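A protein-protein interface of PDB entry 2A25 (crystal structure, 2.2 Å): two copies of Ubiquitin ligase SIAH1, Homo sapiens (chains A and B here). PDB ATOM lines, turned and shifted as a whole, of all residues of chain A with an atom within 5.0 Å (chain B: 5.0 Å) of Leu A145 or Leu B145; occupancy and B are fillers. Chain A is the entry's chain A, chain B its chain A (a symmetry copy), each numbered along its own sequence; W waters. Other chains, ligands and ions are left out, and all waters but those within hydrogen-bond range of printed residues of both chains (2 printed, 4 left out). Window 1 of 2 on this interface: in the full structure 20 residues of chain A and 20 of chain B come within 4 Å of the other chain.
The backbone NH (N) of Thr A146 sits at hydrogen-bond distance from the backbone carbonyl oxygen (O) of Thr B146 (2.8 Å).
OE2 of Glu A137 sits at hydrogen-bond distance from OG1 of Thr A146, at 3.4 Å. The backbone NH (N) of Leu A138 lies within hydrogen-bond range of the backbone carbonyl oxygen (O) of Leu A145, 2.8 Å away. The backbone NH (N) of Trp A147 is in hydrogen-bond range of the backbone carbonyl oxygen (O) of Leu A136, 2.8 Å away. The side-chain carboxylate (OE2) of Glu B137 sits at hydrogen-bond distance from the side-chain hydroxyl (OG1) of Thr B146, 3.4 Å away. N of Leu B138 lies within hydrogen-bond range of O of Leu B145, at 2.8 Å. N of Trp B147 lies within hydrogen-bond range of O of Leu B136 (2.8 Å).
Arg A144 touches Thr B146. Arg A144 touches Trp B147 (O to CA, 3.4 Å). Leu A145 touches Leu B145. CA of Leu A145 touches O of Thr B146 (3.5 Å). Arg B144 touches Thr A146. Thr A146 touches Leu B145. Trp A147 touches Arg B144. Phe B178 touches Trp A147. Trp B147 touches Phe A178.
Glu A137 touches none of the printed residues of chain B. Leu B136 touches none of the printed residues of chain A. Of chain A, only Leu A145 (3.9 Å) and Thr A146 (3.5 Å) come within 4 Å of Leu B145. Printed residues of chain A within 4 Å of Thr B146: Arg A144 (3.8 Å), Leu A145 (3.5 Å) and Thr A146 (2.8 Å). Printed residues of chain A within 4 Å of Trp B147: Arg A144 and Phe A178. The nearest residue of chain B that does not touch Leu A145 is Trp B147 (4.02 Å).
Hydrophobic or aromatic side chains of chain B that line the printed part of chain A: Leu B145, Trp B147 and Phe B178. Along chain B the printed residues that touch a printed residue of chain A span positions 144 to 178. Among the printed residues, 10 pairs touch across the chains. Among the printed residues, no Asp or Glu carboxylate lies within 4 Å of a Lys or Arg side-chain nitrogen of the other chain.
Arg A144 touches Trp B147, and with the chains exchanged Trp A147 touches Arg B144. Leu A145 touches its own counterpart, Leu B145. Thr A146 touches its own counterpart, Thr B146. Trp A147 touches Phe B178, and with the chains exchanged Phe A178 touches Trp B147. Positions printed for both chains: 136, 137, 138, 143, 144, 145, 146, 147, 168, 169, 170, 174 and 178.
Water W1 lies within hydrogen-bond range of OG1 of Thr B146 (2.7 Å), O of Arg B144 (2.8 Å) and O of Thr A146 (3.2 Å). Water W2 lies within hydrogen-bond range of the side-chain hydroxyl of Thr A146 (2.7 Å), the backbone carbonyl oxygen of Arg A144 (2.8 Å) and the backbone carbonyl oxygen of Thr B146 (3.2 Å).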
ATOM      1  N   LEU A 136      16.802 -13.617   7.665  1.00  0.00           N
ATOM      2  CA  LEU A 136      16.629 -12.473   8.594  1.00  0.00           C
ATOM      3  C   LEU A 136      18.007 -12.049   9.035  1.00  0.00           C
ATOM      4  O   LEU A 136      18.771 -12.888   9.455  1.00  0.00           O
ATOM      5  CB  LEU A 136      15.809 -12.885   9.833  1.00  0.00           C
ATOM      6  CG  LEU A 136      14.379 -13.379   9.588  1.00  0.00           C
ATOM      7  CD1 LEU A 136      13.664 -13.757  10.911  1.00  0.00           C
ATOM      8  CD2 LEU A 136      13.557 -12.358   8.803  1.00  0.00           C
ATOM      9  N   GLU A 137      18.336 -10.757   8.926  1.00  0.00           N
ATOM     10  CA  GLU A 137      19.682 -10.284   9.267  1.00  0.00           C
ATOM     11  C   GLU A 137      19.547  -9.084  10.164  1.00  0.00           C
ATOM     12  O   GLU A 137      18.797  -8.157   9.842  1.00  0.00           O
ATOM     13  CB  GLU A 137      20.427  -9.802   8.047  1.00  0.00           C
ATOM     14  CG  GLU A 137      20.988 -10.838   7.116  1.00  0.00           C
ATOM     15  CD  GLU A 137      22.191 -10.308   6.326  1.00  0.00           C
ATOM     16  OE1 GLU A 137      22.286  -9.076   6.103  1.00  0.00           O
ATOM     17  OE2 GLU A 137      23.059 -11.137   5.965  1.00  0.00           O
ATOM     18  N   LEU A 138      20.266  -9.100  11.280  1.00  0.00           N
ATOM     19  CA  LEU A 138      20.456  -7.893  12.059  1.00  0.00           C
ATOM     20  C   LEU A 138      21.859  -7.421  11.716  1.00  0.00           C
ATOM     21  O   LEU A 138      22.788  -8.248  11.603  1.00  0.00           O
ATOM     22  CB  LEU A 138      20.316  -8.171  13.568  1.00  0.00           C
ATOM     23  CG  LEU A 138      19.110  -8.990  14.059  1.00  0.00           C
ATOM     24  CD1 LEU A 138      19.204  -9.259  15.597  1.00  0.00           C
ATOM     25  CD2 LEU A 138      17.755  -8.355  13.674  1.00  0.00           C
ATOM     26  N   ARG A 143      29.042  -6.022  13.416  1.00  0.00           N
ATOM     27  CA  ARG A 143      28.406  -7.249  13.902  1.00  0.00           C
ATOM     28  C   ARG A 143      27.254  -7.574  12.981  1.00  0.00           C
ATOM     29  O   ARG A 143      26.551  -6.667  12.530  1.00  0.00           O
ATOM     30  CB  ARG A 143      27.815  -7.024  15.285  1.00  0.00           C
ATOM     31  CG  ARG A 143      28.826  -6.784  16.360  1.00  0.00           C
ATOM     32  CD  ARG A 143      28.218  -6.215  17.608  1.00  0.00           C
ATOM     33  NE  ARG A 143      29.196  -6.012  18.676  1.00  0.00           N
ATOM     34  CZ  ARG A 143      29.898  -4.895  18.851  1.00  0.00           C
ATOM     35  NH1 ARG A 143      29.758  -3.873  18.016  1.00  0.00           N
ATOM     36  NH2 ARG A 143      30.754  -4.799  19.851  1.00  0.00           N
ATOM     37  N   ARG A 144      27.033  -8.860  12.701  1.00  0.00           N
ATOM     38  CA  ARG A 144      25.888  -9.269  11.883  1.00  0.00           C
ATOM     39  C   ARG A 144      25.361 -10.637  12.337  1.00  0.00           C
ATOM     40  O   ARG A 144      26.139 -11.567  12.501  1.00  0.00           O
ATOM     41  CB  ARG A 144      26.272  -9.301  10.395  1.00  0.00           C
ATOM     42  CG  ARG A 144      25.138  -9.722   9.473  1.00  0.00           C
ATOM     43  CD  ARG A 144      25.204  -9.166   8.042  1.00  0.00           C
ATOM     44  NE  ARG A 144      26.458  -9.498   7.381  1.00  0.00           N
ATOM     45  CZ  ARG A 144      27.153  -8.662   6.625  1.00  0.00           C
ATOM     46  NH1 ARG A 144      26.702  -7.433   6.394  1.00  0.00           N
ATOM     47  NH2 ARG A 144      28.302  -9.060   6.094  1.00  0.00           N
ATOM     48  N   LEU A 145      24.061 -10.718  12.615  1.00  0.00           N
ATOM     49  CA  LEU A 145      23.430 -11.992  12.962  1.00  0.00           C
ATOM     50  C   LEU A 145      22.430 -12.343  11.899  1.00  0.00           C
ATOM     51  O   LEU A 145      21.570 -11.536  11.528  1.00  0.00           O
ATOM     52  CB  LEU A 145      22.757 -11.915  14.334  1.00  0.00           C
ATOM     53  CG  LEU A 145      22.037 -13.142  14.897  1.00  0.00           C
ATOM     54  CD1 LEU A 145      23.005 -14.276  15.253  1.00  0.00           C
ATOM     55  CD2 LEU A 145      21.334 -12.667  16.160  1.00  0.00           C
ATOM     56  N   THR A 146      22.546 -13.559  11.402  1.00  0.00           N
ATOM     57  CA  THR A 146      21.742 -13.982  10.291  1.00  0.00           C
ATOM     58  C   THR A 146      21.064 -15.290  10.575  1.00  0.00           C
ATOM     59  O   THR A 146      21.702 -16.190  11.104  1.00  0.00           O
ATOM     60  CB  THR A 146      22.645 -14.150   9.055  1.00  0.00           C
ATOM     61  OG1 THR A 146      23.317 -12.916   8.799  1.00  0.00           O
ATOM     62  CG2 THR A 146      21.804 -14.326   7.822  1.00  0.00           C
ATOM     63  N   TRP A 147      19.789 -15.407  10.174  1.00  0.00           N
ATOM     64  CA  TRP A 147      19.035 -16.663  10.326  1.00  0.00           C
ATOM     65  C   TRP A 147      18.414 -17.003   8.990  1.00  0.00           C
ATOM     66  O   TRP A 147      17.787 -16.156   8.399  1.00  0.00           O
ATOM     67  CB  TRP A 147      17.901 -16.482  11.356  1.00  0.00           C
ATOM     68  CG  TRP A 147      16.927 -17.659  11.347  1.00  0.00           C
ATOM     69  CD1 TRP A 147      15.662 -17.696  10.773  1.00  0.00           C
ATOM     70  CD2 TRP A 147      17.124 -18.940  11.950  1.00  0.00           C
ATOM     71  NE1 TRP A 147      15.091 -18.931  10.979  1.00  0.00           N
ATOM     72  CE2 TRP A 147      15.954 -19.705  11.713  1.00  0.00           C
ATOM     73  CE3 TRP A 147      18.156 -19.511  12.707  1.00  0.00           C
ATOM     74  CZ2 TRP A 147      15.819 -21.022  12.148  1.00  0.00           C
ATOM     75  CZ3 TRP A 147      18.008 -20.817  13.176  1.00  0.00           C
ATOM     76  CH2 TRP A 147      16.846 -21.564  12.873  1.00  0.00           C
ATOM     77  N   LEU A 168      14.773 -16.743  14.269  1.00  0.00           N
ATOM     78  CA  LEU A 168      15.850 -15.956  14.807  1.00  0.00           C
ATOM     79  C   LEU A 168      15.477 -15.680  16.276  1.00  0.00           C
ATOM     80  O   LEU A 168      14.376 -15.198  16.572  1.00  0.00           O
ATOM     81  CB  LEU A 168      16.018 -14.683  13.999  1.00  0.00           C
ATOM     82  CG  LEU A 168      17.028 -13.630  14.447  1.00  0.00           C
ATOM     83  CD1 LEU A 168      18.432 -14.214  14.466  1.00  0.00           C
ATOM     84  CD2 LEU A 168      16.943 -12.376  13.586  1.00  0.00           C
ATOM     85  N   VAL A 169      16.394 -16.032  17.171  1.00  0.00           N
ATOM     86  CA  VAL A 169      16.237 -15.865  18.593  1.00  0.00           C
ATOM     87  C   VAL A 169      17.397 -15.021  19.067  1.00  0.00           C
ATOM     88  O   VAL A 169      18.575 -15.344  18.827  1.00  0.00           O
ATOM     89  CB  VAL A 169      16.217 -17.212  19.317  1.00  0.00           C
ATOM     90  CG1 VAL A 169      16.242 -17.029  20.840  1.00  0.00           C
ATOM     91  CG2 VAL A 169      14.999 -17.999  18.893  1.00  0.00           C
ATOM     92  N   PHE A 170      17.066 -13.938  19.749  1.00  0.00           N
ATOM     93  CA  PHE A 170      18.085 -13.108  20.333  1.00  0.00           C
ATOM     94  C   PHE A 170      17.501 -12.471  21.567  1.00  0.00           C
ATOM     95  O   PHE A 170      16.291 -12.273  21.666  1.00  0.00           O
ATOM     96  CB  PHE A 170      18.585 -12.053  19.345  1.00  0.00           C
ATOM     97  CG  PHE A 170      17.492 -11.258  18.687  1.00  0.00           C
ATOM     98  CD1 PHE A 170      17.215  -9.958  19.109  1.00  0.00           C
ATOM     99  CD2 PHE A 170      16.738 -11.800  17.638  1.00  0.00           C
ATOM    100  CE1 PHE A 170      16.218  -9.209  18.486  1.00  0.00           C
ATOM    101  CE2 PHE A 170      15.739 -11.082  17.039  1.00  0.00           C
ATOM    102  CZ  PHE A 170      15.481  -9.773  17.463  1.00  0.00           C
ATOM    103  N   ILE A 174      21.557  -8.280  23.059  1.00  0.00           N
ATOM    104  CA  ILE A 174      21.681  -8.349  21.591  1.00  0.00           C
ATOM    105  C   ILE A 174      20.732  -7.377  20.854  1.00  0.00           C
ATOM    106  O   ILE A 174      21.148  -6.682  19.927  1.00  0.00           O
ATOM    107  CB  ILE A 174      21.456  -9.805  21.074  1.00  0.00           C
ATOM    108  CG1 ILE A 174      22.592 -10.726  21.479  1.00  0.00           C
ATOM    109  CG2 ILE A 174      21.335  -9.870  19.530  1.00  0.00           C
ATOM    110  CD1 ILE A 174      22.291 -12.213  21.193  1.00  0.00           C
ATOM    111  N   PHE A 178      21.957  -4.122  18.187  1.00  0.00           N
ATOM    112  CA  PHE A 178      21.665  -3.917  16.766  1.00  0.00           C
ATOM    113  C   PHE A 178      20.709  -2.745  16.531  1.00  0.00           C
ATOM    114  O   PHE A 178      20.586  -2.250  15.402  1.00  0.00           O
ATOM    115  CB  PHE A 178      21.080  -5.196  16.148  1.00  0.00           C
ATOM    116  CG  PHE A 178      22.085  -6.305  16.011  1.00  0.00           C
ATOM    117  CD1 PHE A 178      22.036  -7.415  16.846  1.00  0.00           C
ATOM    118  CD2 PHE A 178      23.110  -6.221  15.070  1.00  0.00           C
ATOM    119  CE1 PHE A 178      22.991  -8.433  16.741  1.00  0.00           C
ATOM    120  CE2 PHE A 178      24.054  -7.239  14.941  1.00  0.00           C
ATOM    121  CZ  PHE A 178      23.996  -8.349  15.782  1.00  0.00           C
ATOM    122  N   LEU B 136      30.897 -17.314  12.125  1.00  0.00           N
ATOM    123  CA  LEU B 136      30.540 -18.615  12.741  1.00  0.00           C
ATOM    124  C   LEU B 136      29.207 -19.026  12.167  1.00  0.00           C
ATOM    125  O   LEU B 136      28.295 -18.231  12.179  1.00  0.00           O
ATOM    126  CB  LEU B 136      30.410 -18.486  14.273  1.00  0.00           C
ATOM    127  CG  LEU B 136      31.660 -18.046  15.041  1.00  0.00           C
ATOM    128  CD1 LEU B 136      31.397 -17.957  16.567  1.00  0.00           C
ATOM    129  CD2 LEU B 136      32.850 -18.956  14.751  1.00  0.00           C
ATOM    130  N   GLU B 137      29.093 -20.254  11.649  1.00  0.00           N
ATOM    131  CA  GLU B 137      27.851 -20.697  11.009  1.00  0.00           C
ATOM    132  C   GLU B 137      27.486 -22.045  11.568  1.00  0.00           C
ATOM    133  O   GLU B 137      28.332 -22.944  11.608  1.00  0.00           O
ATOM    134  CB  GLU B 137      28.033 -20.904   9.526  1.00  0.00           C
ATOM    135  CG  GLU B 137      28.091 -19.684   8.652  1.00  0.00           C
ATOM    136  CD  GLU B 137      27.653 -19.987   7.214  1.00  0.00           C
ATOM    137  OE1 GLU B 137      27.789 -21.150   6.761  1.00  0.00           O
ATOM    138  OE2 GLU B 137      27.134 -19.055   6.557  1.00  0.00           O
ATOM    139  N   LEU B 138      26.237 -22.186  11.996  1.00  0.00           N
ATOM    140  CA  LEU B 138      25.688 -23.500  12.265  1.00  0.00           C
ATOM    141  C   LEU B 138      24.816 -23.814  11.061  1.00  0.00           C
ATOM    142  O   LEU B 138      24.098 -22.925  10.558  1.00  0.00           O
ATOM    143  CB  LEU B 138      24.864 -23.508  13.566  1.00  0.00           C
ATOM    144  CG  LEU B 138      25.468 -22.868  14.828  1.00  0.00           C
ATOM    145  CD1 LEU B 138      24.442 -22.875  16.007  1.00  0.00           C
ATOM    146  CD2 LEU B 138      26.814 -23.505  15.239  1.00  0.00           C
ATOM    147  N   ARG B 143      18.184 -25.049   7.753  1.00  0.00           N
ATOM    148  CA  ARG B 143      18.316 -23.972   8.737  1.00  0.00           C
ATOM    149  C   ARG B 143      19.767 -23.558   8.785  1.00  0.00           C
ATOM    150  O   ARG B 143      20.654 -24.411   8.700  1.00  0.00           O
ATOM    151  CB  ARG B 143      17.956 -24.479  10.125  1.00  0.00           C
ATOM    152  CG  ARG B 143      16.517 -24.847  10.297  1.00  0.00           C
ATOM    153  CD  ARG B 143      16.274 -25.668  11.529  1.00  0.00           C
ATOM    154  NE  ARG B 143      14.864 -25.999  11.723  1.00  0.00           N
ATOM    155  CZ  ARG B 143      14.270 -27.084  11.230  1.00  0.00           C
ATOM    156  NH1 ARG B 143      14.953 -27.945  10.485  1.00  0.00           N
ATOM    157  NH2 ARG B 143      12.990 -27.306  11.465  1.00  0.00           N
ATOM    158  N   ARG B 144      20.033 -22.259   8.935  1.00  0.00           N
ATOM    159  CA  ARG B 144      21.411 -21.781   9.073  1.00  0.00           C
ATOM    160  C   ARG B 144      21.467 -20.553   9.991  1.00  0.00           C
ATOM    161  O   ARG B 144      20.694 -19.621   9.813  1.00  0.00           O
ATOM    162  CB  ARG B 144      22.011 -21.458   7.695  1.00  0.00           C
ATOM    163  CG  ARG B 144      23.443 -20.948   7.748  1.00  0.00           C
ATOM    164  CD  ARG B 144      24.295 -21.231   6.502  1.00  0.00           C
ATOM    165  NE  ARG B 144      23.684 -20.708   5.288  1.00  0.00           N
ATOM    166  CZ  ARG B 144      23.646 -21.349   4.130  1.00  0.00           C
ATOM    167  NH1 ARG B 144      24.219 -22.542   4.004  1.00  0.00           N
ATOM    168  NH2 ARG B 144      23.035 -20.792   3.092  1.00  0.00           N
ATOM    169  N   LEU B 145      22.322 -20.604  11.012  1.00  0.00           N
ATOM    170  CA  LEU B 145      22.531 -19.456  11.893  1.00  0.00           C
ATOM    171  C   LEU B 145      23.947 -18.980  11.744  1.00  0.00           C
ATOM    172  O   LEU B 145      24.903 -19.759  11.834  1.00  0.00           O
ATOM    173  CB  LEU B 145      22.234 -19.820  13.350  1.00  0.00           C
ATOM    174  CG  LEU B 145      22.385 -18.762  14.444  1.00  0.00           C
ATOM    175  CD1 LEU B 145      21.333 -17.653  14.335  1.00  0.00           C
ATOM    176  CD2 LEU B 145      22.202 -19.500  15.762  1.00  0.00           C
ATOM    177  N   THR B 146      24.082 -17.690  11.508  1.00  0.00           N
ATOM    178  CA  THR B 146      25.368 -17.124  11.215  1.00  0.00           C
ATOM    179  C   THR B 146      25.651 -15.934  12.083  1.00  0.00           C
ATOM    180  O   THR B 146      24.769 -15.106  12.267  1.00  0.00           O
ATOM    181  CB  THR B 146      25.395 -16.680   9.741  1.00  0.00           C
ATOM    182  OG1 THR B 146      25.095 -17.804   8.912  1.00  0.00           O
ATOM    183  CG2 THR B 146      26.800 -16.337   9.331  1.00  0.00           C
ATOM    184  N   TRP B 147      26.897 -15.825  12.570  1.00  0.00           N
ATOM    185  CA  TRP B 147      27.323 -14.667  13.373  1.00  0.00           C
ATOM    186  C   TRP B 147      28.606 -14.130  12.779  1.00  0.00           C
ATOM    187  O   TRP B 147      29.514 -14.893  12.551  1.00  0.00           O
ATOM    188  CB  TRP B 147      27.605 -15.100  14.827  1.00  0.00           C
ATOM    189  CG  TRP B 147      28.308 -14.003  15.624  1.00  0.00           C
ATOM    190  CD1 TRP B 147      29.656 -13.942  15.956  1.00  0.00           C
ATOM    191  CD2 TRP B 147      27.706 -12.843  16.201  1.00  0.00           C
ATOM    192  NE1 TRP B 147      29.906 -12.802  16.686  1.00  0.00           N
ATOM    193  CE2 TRP B 147      28.729 -12.122  16.869  1.00  0.00           C
ATOM    194  CE3 TRP B 147      26.394 -12.355  16.262  1.00  0.00           C
ATOM    195  CZ2 TRP B 147      28.489 -10.916  17.524  1.00  0.00           C
ATOM    196  CZ3 TRP B 147      26.145 -11.167  16.950  1.00  0.00           C
ATOM    197  CH2 TRP B 147      27.202 -10.451  17.558  1.00  0.00           C
ATOM    198  N   LEU B 168      28.292 -15.564  19.028  1.00  0.00           N
ATOM    199  CA  LEU B 168      27.161 -16.366  18.646  1.00  0.00           C
ATOM    200  C   LEU B 168      26.580 -16.926  19.959  1.00  0.00           C
ATOM    201  O   LEU B 168      27.302 -17.520  20.770  1.00  0.00           O
ATOM    202  CB  LEU B 168      27.599 -17.460  17.690  1.00  0.00           C
ATOM    203  CG  LEU B 168      26.593 -18.511  17.231  1.00  0.00           C
ATOM    204  CD1 LEU B 168      25.433 -17.855  16.498  1.00  0.00           C
ATOM    205  CD2 LEU B 168      27.261 -19.592  16.391  1.00  0.00           C
ATOM    206  N   VAL B 169      25.288 -16.685  20.156  1.00  0.00           N
ATOM    207  CA  VAL B 169      24.558 -17.116  21.321  1.00  0.00           C
ATOM    208  C   VAL B 169      23.404 -17.957  20.829  1.00  0.00           C
ATOM    209  O   VAL B 169      22.598 -17.524  19.985  1.00  0.00           O
ATOM    210  CB  VAL B 169      24.050 -15.925  22.136  1.00  0.00           C
ATOM    211  CG1 VAL B 169      23.115 -16.378  23.264  1.00  0.00           C
ATOM    212  CG2 VAL B 169      25.223 -15.151  22.691  1.00  0.00           C
ATOM    213  N   PHE B 170      23.318 -19.164  21.362  1.00  0.00           N
ATOM    214  CA  PHE B 170      22.208 -20.022  21.044  1.00  0.00           C
ATOM    215  C   PHE B 170      21.959 -20.906  22.238  1.00  0.00           C
ATOM    216  O   PHE B 170      22.869 -21.193  23.014  1.00  0.00           O
ATOM    217  CB  PHE B 170      22.479 -20.848  19.786  1.00  0.00           C
ATOM    218  CG  PHE B 170      23.793 -21.577  19.798  1.00  0.00           C
ATOM    219  CD1 PHE B 170      23.836 -22.947  20.058  1.00  0.00           C
ATOM    220  CD2 PHE B 170      24.994 -20.902  19.544  1.00  0.00           C
ATOM    221  CE1 PHE B 170      25.050 -23.631  20.048  1.00  0.00           C
ATOM    222  CE2 PHE B 170      26.193 -21.561  19.559  1.00  0.00           C
ATOM    223  CZ  PHE B 170      26.220 -22.938  19.807  1.00  0.00           C
ATOM    224  N   ILE B 174      18.101 -25.037  20.167  1.00  0.00           N
ATOM    225  CA  ILE B 174      18.892 -24.697  18.969  1.00  0.00           C
ATOM    226  C   ILE B 174      20.152 -25.577  18.802  1.00  0.00           C
ATOM    227  O   ILE B 174      20.429 -26.066  17.707  1.00  0.00           O
ATOM    228  CB  ILE B 174      19.294 -23.188  18.970  1.00  0.00           C
ATOM    229  CG1 ILE B 174      18.092 -22.287  18.759  1.00  0.00           C
ATOM    230  CG2 ILE B 174      20.325 -22.853  17.861  1.00  0.00           C
ATOM    231  CD1 ILE B 174      18.412 -20.795  18.988  1.00  0.00           C
ATOM    232  N   PHE B 178      21.006 -28.215  15.408  1.00  0.00           N
ATOM    233  CA  PHE B 178      22.114 -28.178  14.450  1.00  0.00           C
ATOM    234  C   PHE B 178      23.086 -29.345  14.638  1.00  0.00           C
ATOM    235  O   PHE B 178      23.901 -29.635  13.751  1.00  0.00           O
ATOM    236  CB  PHE B 178      22.874 -26.847  14.558  1.00  0.00           C
ATOM    237  CG  PHE B 178      22.093 -25.672  14.042  1.00  0.00           C
ATOM    238  CD1 PHE B 178      21.555 -24.736  14.918  1.00  0.00           C
ATOM    239  CD2 PHE B 178      21.860 -25.520  12.676  1.00  0.00           C
ATOM    240  CE1 PHE B 178      20.800 -23.658  14.439  1.00  0.00           C
ATOM    241  CE2 PHE B 178      21.128 -24.439  12.186  1.00  0.00           C
ATOM    242  CZ  PHE B 178      20.594 -23.505  13.071  1.00  0.00           C
HETATM  243  O   HOH W   1      22.419 -17.892   8.476  1.00  0.00           O
HETATM  244  O   HOH W   2      25.694 -12.917  10.106  1.00  0.00           O
